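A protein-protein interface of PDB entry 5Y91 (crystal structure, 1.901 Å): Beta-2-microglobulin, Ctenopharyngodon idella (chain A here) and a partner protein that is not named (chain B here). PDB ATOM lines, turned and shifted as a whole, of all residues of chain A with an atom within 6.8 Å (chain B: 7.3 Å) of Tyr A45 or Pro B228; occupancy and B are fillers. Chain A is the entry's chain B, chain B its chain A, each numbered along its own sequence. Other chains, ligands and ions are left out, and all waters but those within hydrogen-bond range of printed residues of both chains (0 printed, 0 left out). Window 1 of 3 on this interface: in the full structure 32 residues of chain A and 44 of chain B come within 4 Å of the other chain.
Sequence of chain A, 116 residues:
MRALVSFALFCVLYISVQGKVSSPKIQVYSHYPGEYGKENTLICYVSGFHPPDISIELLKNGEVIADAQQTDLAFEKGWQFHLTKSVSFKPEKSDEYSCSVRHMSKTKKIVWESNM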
ATOM      1  N   LYS A  25      31.376 -26.650 -25.132  1.00  0.00           N
ATOM      2  CA  LYS A  25      29.971 -26.356 -24.905  1.00  0.00           C
ATOM      3  C   LYS A  25      29.935 -25.217 -23.898  1.00  0.00           C
ATOM      4  O   LYS A  25      30.693 -25.216 -22.928  1.00  0.00           O
ATOM      5  CB  LYS A  25      29.213 -27.564 -24.355  1.00  0.00           C
ATOM      6  CG  LYS A  25      27.715 -27.309 -24.212  1.00  0.00           C
ATOM      7  CD  LYS A  25      27.059 -28.226 -23.191  1.00  0.00           C
ATOM      8  CE  LYS A  25      26.940 -29.646 -23.700  1.00  0.00           C
ATOM      9  NZ  LYS A  25      26.224 -30.512 -22.723  1.00  0.00           N
ATOM     10  N   ILE A  26      29.067 -24.241 -24.137  1.00  0.00           N
ATOM     11  CA  ILE A  26      29.005 -23.063 -23.289  1.00  0.00           C
ATOM     12  C   ILE A  26      27.586 -22.865 -22.789  1.00  0.00           C
ATOM     13  O   ILE A  26      26.649 -22.775 -23.580  1.00  0.00           O
ATOM     14  CB  ILE A  26      29.450 -21.804 -24.054  1.00  0.00           C
ATOM     15  CG1 ILE A  26      30.798 -22.045 -24.739  1.00  0.00           C
ATOM     16  CG2 ILE A  26      29.520 -20.602 -23.120  1.00  0.00           C
ATOM     17  CD1 ILE A  26      31.238 -20.914 -25.633  1.00  0.00           C
ATOM     18  N   GLN A  27      27.428 -22.806 -21.474  1.00  0.00           N
ATOM     19  CA  GLN A  27      26.116 -22.597 -20.887  1.00  0.00           C
ATOM     20  C   GLN A  27      26.162 -21.447 -19.889  1.00  0.00           C
ATOM     21  O   GLN A  27      26.933 -21.470 -18.933  1.00  0.00           O
ATOM     22  CB  GLN A  27      25.608 -23.884 -20.235  1.00  0.00           C
ATOM     23  CG  GLN A  27      25.424 -25.026 -21.230  1.00  0.00           C
ATOM     24  CD  GLN A  27      25.014 -26.328 -20.571  1.00  0.00           C
ATOM     25  OE1 GLN A  27      23.835 -26.684 -20.553  1.00  0.00           O
ATOM     26  NE2 GLN A  27      25.990 -27.051 -20.030  1.00  0.00           N
ATOM     27  N   VAL A  28      25.336 -20.436 -20.133  1.00  0.00           N
ATOM     28  CA  VAL A  28      25.302 -19.249 -19.289  1.00  0.00           C
ATOM     29  C   VAL A  28      23.981 -19.182 -18.539  1.00  0.00           C
ATOM     30  O   VAL A  28      22.911 -19.305 -19.138  1.00  0.00           O
ATOM     31  CB  VAL A  28      25.486 -17.968 -20.119  1.00  0.00           C
ATOM     32  CG1 VAL A  28      25.720 -16.770 -19.209  1.00  0.00           C
ATOM     33  CG2 VAL A  28      26.640 -18.136 -21.086  1.00  0.00           C
ATOM     34  N   TYR A  29      24.062 -18.991 -17.225  1.00  0.00           N
ATOM     35  CA  TYR A  29      22.876 -18.968 -16.381  1.00  0.00           C
ATOM     36  C   TYR A  29      23.166 -18.248 -15.074  1.00  0.00           C
ATOM     37  O   TYR A  29      24.312 -17.911 -14.783  1.00  0.00           O
ATOM     38  CB  TYR A  29      22.393 -20.396 -16.096  1.00  0.00           C
ATOM     39  CG  TYR A  29      23.484 -21.336 -15.617  1.00  0.00           C
ATOM     40  CD1 TYR A  29      24.346 -21.942 -16.522  1.00  0.00           C
ATOM     41  CD2 TYR A  29      23.643 -21.627 -14.266  1.00  0.00           C
ATOM     42  CE1 TYR A  29      25.342 -22.802 -16.101  1.00  0.00           C
ATOM     43  CE2 TYR A  29      24.641 -22.490 -13.832  1.00  0.00           C
ATOM     44  CZ  TYR A  29      25.486 -23.075 -14.758  1.00  0.00           C
ATOM     45  OH  TYR A  29      26.481 -23.933 -14.347  1.00  0.00           O
ATOM     46  N   ILE A  43      26.784 -17.164 -14.028  1.00  0.00           N
ATOM     47  CA  ILE A  43      27.586 -18.374 -14.149  1.00  0.00           C
ATOM     48  C   ILE A  43      27.770 -18.781 -15.603  1.00  0.00           C
ATOM     49  O   ILE A  43      26.825 -18.766 -16.390  1.00  0.00           O
ATOM     50  CB  ILE A  43      26.941 -19.554 -13.381  1.00  0.00           C
ATOM     51  CG1 ILE A  43      26.761 -19.195 -11.906  1.00  0.00           C
ATOM     52  CG2 ILE A  43      27.782 -20.818 -13.527  1.00  0.00           C
ATOM     53  CD1 ILE A  43      26.041 -20.264 -11.100  1.00  0.00           C
ATOM     54  N   CYS A  44      28.999 -19.137 -15.956  1.00  0.00           N
ATOM     55  CA  CYS A  44      29.287 -19.648 -17.285  1.00  0.00           C
ATOM     56  C   CYS A  44      29.992 -20.987 -17.143  1.00  0.00           C
ATOM     57  O   CYS A  44      31.116 -21.056 -16.645  1.00  0.00           O
ATOM     58  CB  CYS A  44      30.152 -18.663 -18.072  1.00  0.00           C
ATOM     59  SG  CYS A  44      30.402 -19.124 -19.805  1.00  0.00           S
ATOM     60  N   TYR A  45      29.314 -22.049 -17.563  1.00  0.00           N
ATOM     61  CA  TYR A  45      29.861 -23.396 -17.479  1.00  0.00           C
ATOM     62  C   TYR A  45      30.372 -23.826 -18.846  1.00  0.00           C
ATOM     63  O   TYR A  45      29.598 -23.972 -19.793  1.00  0.00           O
ATOM     64  CB  TYR A  45      28.798 -24.369 -16.970  1.00  0.00           C
ATOM     65  CG  TYR A  45      29.281 -25.792 -16.793  1.00  0.00           C
ATOM     66  CD1 TYR A  45      30.383 -26.080 -15.997  1.00  0.00           C
ATOM     67  CD2 TYR A  45      28.620 -26.848 -17.404  1.00  0.00           C
ATOM     68  CE1 TYR A  45      30.825 -27.384 -15.830  1.00  0.00           C
ATOM     69  CE2 TYR A  45      29.052 -28.153 -17.242  1.00  0.00           C
ATOM     70  CZ  TYR A  45      30.154 -28.414 -16.456  1.00  0.00           C
ATOM     71  OH  TYR A  45      30.582 -29.711 -16.293  1.00  0.00           O
ATOM     72  N   VAL A  46      31.682 -24.018 -18.939  1.00  0.00           N
ATOM     73  CA  VAL A  46      32.338 -24.345 -20.199  1.00  0.00           C
ATOM     74  C   VAL A  46      32.911 -25.756 -20.116  1.00  0.00           C
ATOM     75  O   VAL A  46      33.781 -26.022 -19.289  1.00  0.00           O
ATOM     76  CB  VAL A  46      33.474 -23.351 -20.490  1.00  0.00           C
ATOM     77  CG1 VAL A  46      34.130 -23.659 -21.833  1.00  0.00           C
ATOM     78  CG2 VAL A  46      32.946 -21.918 -20.457  1.00  0.00           C
ATOM     79  N   SER A  47      32.425 -26.655 -20.966  1.00  0.00           N
ATOM     80  CA  SER A  47      32.772 -28.070 -20.847  1.00  0.00           C
ATOM     81  C   SER A  47      33.081 -28.750 -22.179  1.00  0.00           C
ATOM     82  O   SER A  47      32.880 -28.179 -23.250  1.00  0.00           O
ATOM     83  CB  SER A  47      31.647 -28.825 -20.133  1.00  0.00           C
ATOM     84  OG  SER A  47      30.421 -28.697 -20.832  1.00  0.00           O
ATOM     85  N   GLY A  48      33.581 -29.979 -22.089  1.00  0.00           N
ATOM     86  CA  GLY A  48      33.807 -30.819 -23.251  1.00  0.00           C
ATOM     87  C   GLY A  48      34.786 -30.283 -24.276  1.00  0.00           C
ATOM     88  O   GLY A  48      34.663 -30.582 -25.464  1.00  0.00           O
ATOM     89  N   ILE A  56      38.105 -17.448 -20.882  1.00  0.00           N
ATOM     90  CA  ILE A  56      36.707 -17.218 -20.543  1.00  0.00           C
ATOM     91  C   ILE A  56      36.554 -15.887 -19.820  1.00  0.00           C
ATOM     92  O   ILE A  56      37.313 -15.577 -18.904  1.00  0.00           O
ATOM     93  CB  ILE A  56      36.149 -18.345 -19.652  1.00  0.00           C
ATOM     94  CG1 ILE A  56      36.441 -19.711 -20.276  1.00  0.00           C
ATOM     95  CG2 ILE A  56      34.652 -18.152 -19.424  1.00  0.00           C
ATOM     96  CD1 ILE A  56      36.223 -20.878 -19.330  1.00  0.00           C
ATOM     97  N   GLU A  76      36.122 -34.602 -16.598  1.00  0.00           N
ATOM     98  CA  GLU A  76      35.247 -35.700 -16.209  1.00  0.00           C
ATOM     99  C   GLU A  76      35.682 -36.993 -16.884  1.00  0.00           C
ATOM    100  O   GLU A  76      36.608 -36.995 -17.697  1.00  0.00           O
ATOM    101  CB  GLU A  76      33.802 -35.374 -16.587  1.00  0.00           C
ATOM    102  CG  GLU A  76      33.230 -34.173 -15.850  1.00  0.00           C
ATOM    103  CD  GLU A  76      32.007 -33.589 -16.537  1.00  0.00           C
ATOM    104  OE1 GLU A  76      32.081 -33.308 -17.753  1.00  0.00           O
ATOM    105  OE2 GLU A  76      30.974 -33.404 -15.860  1.00  0.00           O
ATOM    106  N   PHE A  81      37.615 -31.609 -20.595  1.00  0.00           N
ATOM    107  CA  PHE A  81      37.810 -30.593 -19.570  1.00  0.00           C
ATOM    108  C   PHE A  81      36.548 -29.785 -19.306  1.00  0.00           C
ATOM    109  O   PHE A  81      35.680 -29.669 -20.169  1.00  0.00           O
ATOM    110  CB  PHE A  81      38.940 -29.645 -19.973  1.00  0.00           C
ATOM    111  CG  PHE A  81      40.279 -30.310 -20.071  1.00  0.00           C
ATOM    112  CD1 PHE A  81      41.022 -30.558 -18.932  1.00  0.00           C
ATOM    113  CD2 PHE A  81      40.792 -30.687 -21.300  1.00  0.00           C
ATOM    114  CE1 PHE A  81      42.255 -31.174 -19.012  1.00  0.00           C
ATOM    115  CE2 PHE A  81      42.029 -31.302 -21.390  1.00  0.00           C
ATOM    116  CZ  PHE A  81      42.761 -31.545 -20.244  1.00  0.00           C
ATOM    117  N   HIS A  82      36.454 -29.230 -18.104  1.00  0.00           N
ATOM    118  CA  HIS A  82      35.379 -28.305 -17.782  1.00  0.00           C
ATOM    119  C   HIS A  82      35.866 -27.215 -16.837  1.00  0.00           C
ATOM    120  O   HIS A  82      36.749 -27.439 -16.011  1.00  0.00           O
ATOM    121  CB  HIS A  82      34.168 -29.036 -17.193  1.00  0.00           C
ATOM    122  CG  HIS A  82      34.441 -29.715 -15.888  1.00  0.00           C
ATOM    123  ND1 HIS A  82      34.465 -29.037 -14.687  1.00  0.00           N
ATOM    124  CD2 HIS A  82      34.687 -31.013 -15.592  1.00  0.00           C
ATOM    125  CE1 HIS A  82      34.721 -29.888 -13.709  1.00  0.00           C
ATOM    126  NE2 HIS A  82      34.860 -31.093 -14.231  1.00  0.00           N
ATOM    127  N   LEU A  83      35.294 -26.027 -16.991  1.00  0.00           N
ATOM    128  CA  LEU A  83      35.634 -24.883 -16.162  1.00  0.00           C
ATOM    129  C   LEU A  83      34.367 -24.105 -15.851  1.00  0.00           C
ATOM    130  O   LEU A  83      33.433 -24.076 -16.652  1.00  0.00           O
ATOM    131  CB  LEU A  83      36.619 -23.964 -16.887  1.00  0.00           C
ATOM    132  CG  LEU A  83      38.047 -24.463 -17.110  1.00  0.00           C
ATOM    133  CD1 LEU A  83      38.780 -23.532 -18.061  1.00  0.00           C
ATOM    134  CD2 LEU A  83      38.789 -24.576 -15.784  1.00  0.00           C
ATOM    135  N   THR A  84      34.338 -23.473 -14.686  1.00  0.00           N
ATOM    136  CA  THR A  84      33.223 -22.614 -14.327  1.00  0.00           C
ATOM    137  C   THR A  84      33.734 -21.221 -13.992  1.00  0.00           C
ATOM    138  O   THR A  84      34.629 -21.060 -13.166  1.00  0.00           O
ATOM    139  CB  THR A  84      32.435 -23.178 -13.129  1.00  0.00           C
ATOM    140  OG1 THR A  84      31.836 -24.427 -13.496  1.00  0.00           O
ATOM    141  CG2 THR A  84      31.341 -22.207 -12.704  1.00  0.00           C
ATOM    142  N   LYS A  85      33.179 -20.215 -14.656  1.00  0.00           N
ATOM    143  CA  LYS A  85      33.499 -18.837 -14.324  1.00  0.00           C
ATOM    144  C   LYS A  85      32.249 -18.168 -13.784  1.00  0.00           C
ATOM    145  O   LYS A  85      31.169 -18.306 -14.357  1.00  0.00           O
ATOM    146  CB  LYS A  85      34.025 -18.083 -15.544  1.00  0.00           C
ATOM    147  CG  LYS A  85      34.665 -16.750 -15.204  1.00  0.00           C
ATOM    148  CD  LYS A  85      35.926 -16.544 -16.017  1.00  0.00           C
ATOM    149  CE  LYS A  85      36.782 -15.437 -15.444  1.00  0.00           C
ATOM    150  NZ  LYS A  85      38.076 -15.346 -16.172  1.00  0.00           N
ATOM    151  N   CYS A  99      28.800 -14.380 -21.802  1.00  0.00           N
ATOM    152  CA  CYS A  99      30.043 -15.093 -21.553  1.00  0.00           C
ATOM    153  C   CYS A  99      30.784 -15.257 -22.871  1.00  0.00           C
ATOM    154  O   CYS A  99      30.259 -15.851 -23.814  1.00  0.00           O
ATOM    155  CB  CYS A  99      29.759 -16.466 -20.944  1.00  0.00           C
ATOM    156  SG  CYS A  99      31.233 -17.462 -20.632  1.00  0.00           S
ATOM    157  N   GLU B 225      19.499 -29.613 -18.712  1.00  0.00           N
ATOM    158  CA  GLU B 225      20.593 -30.347 -18.084  1.00  0.00           C
ATOM    159  C   GLU B 225      20.794 -29.957 -16.628  1.00  0.00           C
ATOM    160  O   GLU B 225      20.529 -28.820 -16.238  1.00  0.00           O
ATOM    161  CB  GLU B 225      21.904 -30.105 -18.838  1.00  0.00           C
ATOM    162  CG  GLU B 225      21.918 -30.595 -20.274  1.00  0.00           C
ATOM    163  CD  GLU B 225      23.254 -30.345 -20.954  1.00  0.00           C
ATOM    164  OE1 GLU B 225      23.340 -30.519 -22.188  1.00  0.00           O
ATOM    165  OE2 GLU B 225      24.221 -29.973 -20.255  1.00  0.00           O
ATOM    166  N   LEU B 226      21.268 -30.908 -15.828  1.00  0.00           N
ATOM    167  CA  LEU B 226      21.722 -30.619 -14.475  1.00  0.00           C
ATOM    168  C   LEU B 226      22.949 -29.723 -14.562  1.00  0.00           C
ATOM    169  O   LEU B 226      23.913 -30.051 -15.255  1.00  0.00           O
ATOM    170  CB  LEU B 226      22.079 -31.915 -13.749  1.00  0.00           C
ATOM    171  CG  LEU B 226      22.751 -31.776 -12.383  1.00  0.00           C
ATOM    172  CD1 LEU B 226      21.774 -31.223 -11.349  1.00  0.00           C
ATOM    173  CD2 LEU B 226      23.322 -33.110 -11.934  1.00  0.00           C
ATOM    174  N   LEU B 227      22.914 -28.593 -13.865  1.00  0.00           N
ATOM    175  CA  LEU B 227      24.005 -27.626 -13.932  1.00  0.00           C
ATOM    176  C   LEU B 227      24.578 -27.324 -12.553  1.00  0.00           C
ATOM    177  O   LEU B 227      23.853 -27.313 -11.560  1.00  0.00           O
ATOM    178  CB  LEU B 227      23.526 -26.330 -14.590  1.00  0.00           C
ATOM    179  CG  LEU B 227      23.086 -26.424 -16.052  1.00  0.00           C
ATOM    180  CD1 LEU B 227      22.401 -25.135 -16.493  1.00  0.00           C
ATOM    181  CD2 LEU B 227      24.269 -26.748 -16.952  1.00  0.00           C
ATOM    182  N   PRO B 228      25.891 -27.068 -12.488  1.00  0.00           N
ATOM    183  CA  PRO B 228      26.520 -26.747 -11.207  1.00  0.00           C
ATOM    184  C   PRO B 228      26.393 -25.267 -10.857  1.00  0.00           C
ATOM    185  O   PRO B 228      26.534 -24.411 -11.727  1.00  0.00           O
ATOM    186  CB  PRO B 228      27.990 -27.094 -11.445  1.00  0.00           C
ATOM    187  CG  PRO B 228      28.193 -26.959 -12.924  1.00  0.00           C
ATOM    188  CD  PRO B 228      26.851 -27.053 -13.605  1.00  0.00           C
ATOM    189  N   ASN B 229      26.118 -24.979  -9.591  1.00  0.00           N
ATOM    190  CA  ASN B 229      26.203 -23.614  -9.094  1.00  0.00           C
ATOM    191  C   ASN B 229      27.632 -23.332  -8.648  1.00  0.00           C
ATOM    192  O   ASN B 229      28.480 -24.226  -8.665  1.00  0.00           O
ATOM    193  CB  ASN B 229      25.216 -23.383  -7.946  1.00  0.00           C
ATOM    194  CG  ASN B 229      23.790 -23.203  -8.433  1.00  0.00           C
ATOM    195  OD1 ASN B 229      23.560 -22.750  -9.554  1.00  0.00           O
ATOM    196  ND2 ASN B 229      22.824 -23.549  -7.590  1.00  0.00           N
ATOM    197  N   GLU B 230      27.896 -22.095  -8.246  1.00  0.00           N
ATOM    198  CA  GLU B 230      29.249 -21.687  -7.880  1.00  0.00           C
ATOM    199  C   GLU B 230      29.643 -22.125  -6.471  1.00  0.00           C
ATOM    200  O   GLU B 230      30.815 -22.066  -6.102  1.00  0.00           O
ATOM    201  CB  GLU B 230      29.397 -20.169  -8.012  1.00  0.00           C
ATOM    202  CG  GLU B 230      28.913 -19.376  -6.802  1.00  0.00           C
ATOM    203  CD  GLU B 230      27.406 -19.422  -6.608  1.00  0.00           C
ATOM    204  OE1 GLU B 230      26.932 -18.904  -5.574  1.00  0.00           O
ATOM    205  OE2 GLU B 230      26.693 -19.965  -7.481  1.00  0.00           O
ATOM    206  N   ASP B 231      28.665 -22.568  -5.687  1.00  0.00           N
ATOM    207  CA  ASP B 231      28.900 -22.862  -4.277  1.00  0.00           C
ATOM    208  C   ASP B 231      28.853 -24.352  -3.945  1.00  0.00           C
ATOM    209  O   ASP B 231      28.821 -24.726  -2.776  1.00  0.00           O
ATOM    210  CB  ASP B 231      27.901 -22.102  -3.402  1.00  0.00           C
ATOM    211  CG  ASP B 231      26.460 -22.491  -3.685  1.00  0.00           C
ATOM    212  OD1 ASP B 231      26.216 -23.234  -4.661  1.00  0.00           O
ATOM    213  OD2 ASP B 231      25.569 -22.049  -2.930  1.00  0.00           O
ATOM    214  N   GLY B 232      28.852 -25.198  -4.968  1.00  0.00           N
ATOM    215  CA  GLY B 232      28.815 -26.631  -4.753  1.00  0.00           C
ATOM    216  C   GLY B 232      27.421 -27.220  -4.840  1.00  0.00           C
ATOM    217  O   GLY B 232      27.259 -28.441  -4.848  1.00  0.00           O
ATOM    218  N   SER B 233      26.409 -26.357  -4.895  1.00  0.00           N
ATOM    219  CA  SER B 233      25.039 -26.815  -5.090  1.00  0.00           C
ATOM    220  C   SER B 233      24.755 -26.980  -6.577  1.00  0.00           C
ATOM    221  O   SER B 233      25.633 -26.768  -7.412  1.00  0.00           O
ATOM    222  CB  SER B 233      24.034 -25.844  -4.463  1.00  0.00           C
ATOM    223  OG  SER B 233      23.983 -24.623  -5.181  1.00  0.00           O
ATOM    224  N   PHE B 234      23.524 -27.357  -6.905  1.00  0.00           N
ATOM    225  CA  PHE B 234      23.155 -27.617  -8.289  1.00  0.00           C
ATOM    226  C   PHE B 234      21.839 -26.952  -8.657  1.00  0.00           C
ATOM    227  O   PHE B 234      21.086 -26.511  -7.789  1.00  0.00           O
ATOM    228  CB  PHE B 234      23.057 -29.124  -8.538  1.00  0.00           C
ATOM    229  CG  PHE B 234      24.364 -29.846  -8.382  1.00  0.00           C
ATOM    230  CD1 PHE B 234      24.800 -30.256  -7.132  1.00  0.00           C
ATOM    231  CD2 PHE B 234      25.158 -30.111  -9.484  1.00  0.00           C
ATOM    232  CE1 PHE B 234      26.003 -30.916  -6.984  1.00  0.00           C
ATOM    233  CE2 PHE B 234      26.365 -30.772  -9.343  1.00  0.00           C
ATOM    234  CZ  PHE B 234      26.787 -31.175  -8.091  1.00  0.00           C
ATOM    235  N   GLN B 235      21.567 -26.882  -9.953  1.00  0.00           N
ATOM    236  CA  GLN B 235      20.277 -26.409 -10.422  1.00  0.00           C
ATOM    237  C   GLN B 235      19.859 -27.181 -11.662  1.00  0.00           C
ATOM    238  O   GLN B 235      20.679 -27.830 -12.308  1.00  0.00           O
ATOM    239  CB  GLN B 235      20.314 -24.911 -10.716  1.00  0.00           C
ATOM    240  CG  GLN B 235      21.177 -24.527 -11.905  1.00  0.00           C
ATOM    241  CD  GLN B 235      20.982 -23.081 -12.308  1.00  0.00           C
ATOM    242  OE1 GLN B 235      20.236 -22.781 -13.237  1.00  0.00           O
ATOM    243  NE2 GLN B 235      21.643 -22.173 -11.599  1.00  0.00           N
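The side-chain carboxylate (OE1) of Glu B225 is in salt-bridge range of the side-chain amino group (NZ) of Lys A25. The side-chain amide oxygen of Gln A27 sits close to the side-chain carboxylate of Glu B225 (3.3 Å). OH of Tyr A29 sits at hydrogen-bond distance from O of Pro B228 (2.7 Å).
The backbone NH (N) of Gln B235 sits at hydrogen-bond distance from the backbone carbonyl oxygen (O) of Leu B227 (2.8 Å). ND2 of Asn B229 sits at hydrogen-bond distance from OG of Ser B233 (2.9 Å). ND2 of Asn B229 sits at hydrogen-bond distance from O of Phe B234 (3.4 Å). The backbone carbonyl oxygen (O) of Ser A47 sits at hydrogen-bond distance from the backbone NH (N) of Lys A25 (2.9 Å). The backbone carbonyl oxygen of Gln A27 lies within hydrogen-bond range of the backbone NH of Tyr A45, at 2.8 Å. The side-chain sulfur of Cys A99 forms a disulfide with the side-chain sulfur of Cys A44, at 2.0 Å.
Among the printed residues, pairs that only touch across the chains: Gln A27 with Leu B227, Tyr A29 with Leu B227, Tyr A29 with Gln B235, Ile A43 with Asn B229, Ile A43 with Glu B230 and Tyr A45 with Pro B228.
Of the printed residues of chain B, Tyr A29 touches Leu B227 (3.7 Å), Pro B228 (2.7 Å) and Gln B235 (3.4 Å). Tyr A45 touches just one residue of chain B: Pro B228 (3.9 Å). Printed residues of chain A within 4 Å of Leu B227: Gln A27 (3.5 Å) and Tyr A29 (3.7 Å). Of chain A, only Tyr A29 and Tyr A45 come within 4 Å of Pro B228. Printed residues of chain A within 4 Å of Asn B229: Ile A43. The nearest residue of chain B that does not touch Tyr A45 is Leu B227 (4.4 Å). The nearest residue of chain A that does not touch Pro B228 is Ile A43 (4.2 Å). The nearest printed residue of chain A that does not touch Glu B225 is Tyr A45 (6.0 Å).
Printed residues of chain A that touch a printed residue of chain B: Lys A25, Gln A27, Tyr A29, Ile A43 and Tyr A45. Hydrophobic or aromatic side chains of chain A that line the printed part of chain B: Tyr A29, Ile A43 and Tyr A45. Along chain A the printed residues that touch a printed residue of chain B span positions 25 to 45. Hydrophobic or aromatic side chains of chain B that line the printed part of chain A: Leu B227 and Pro B228. Among the printed residues, 9 pairs touch across the chains.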
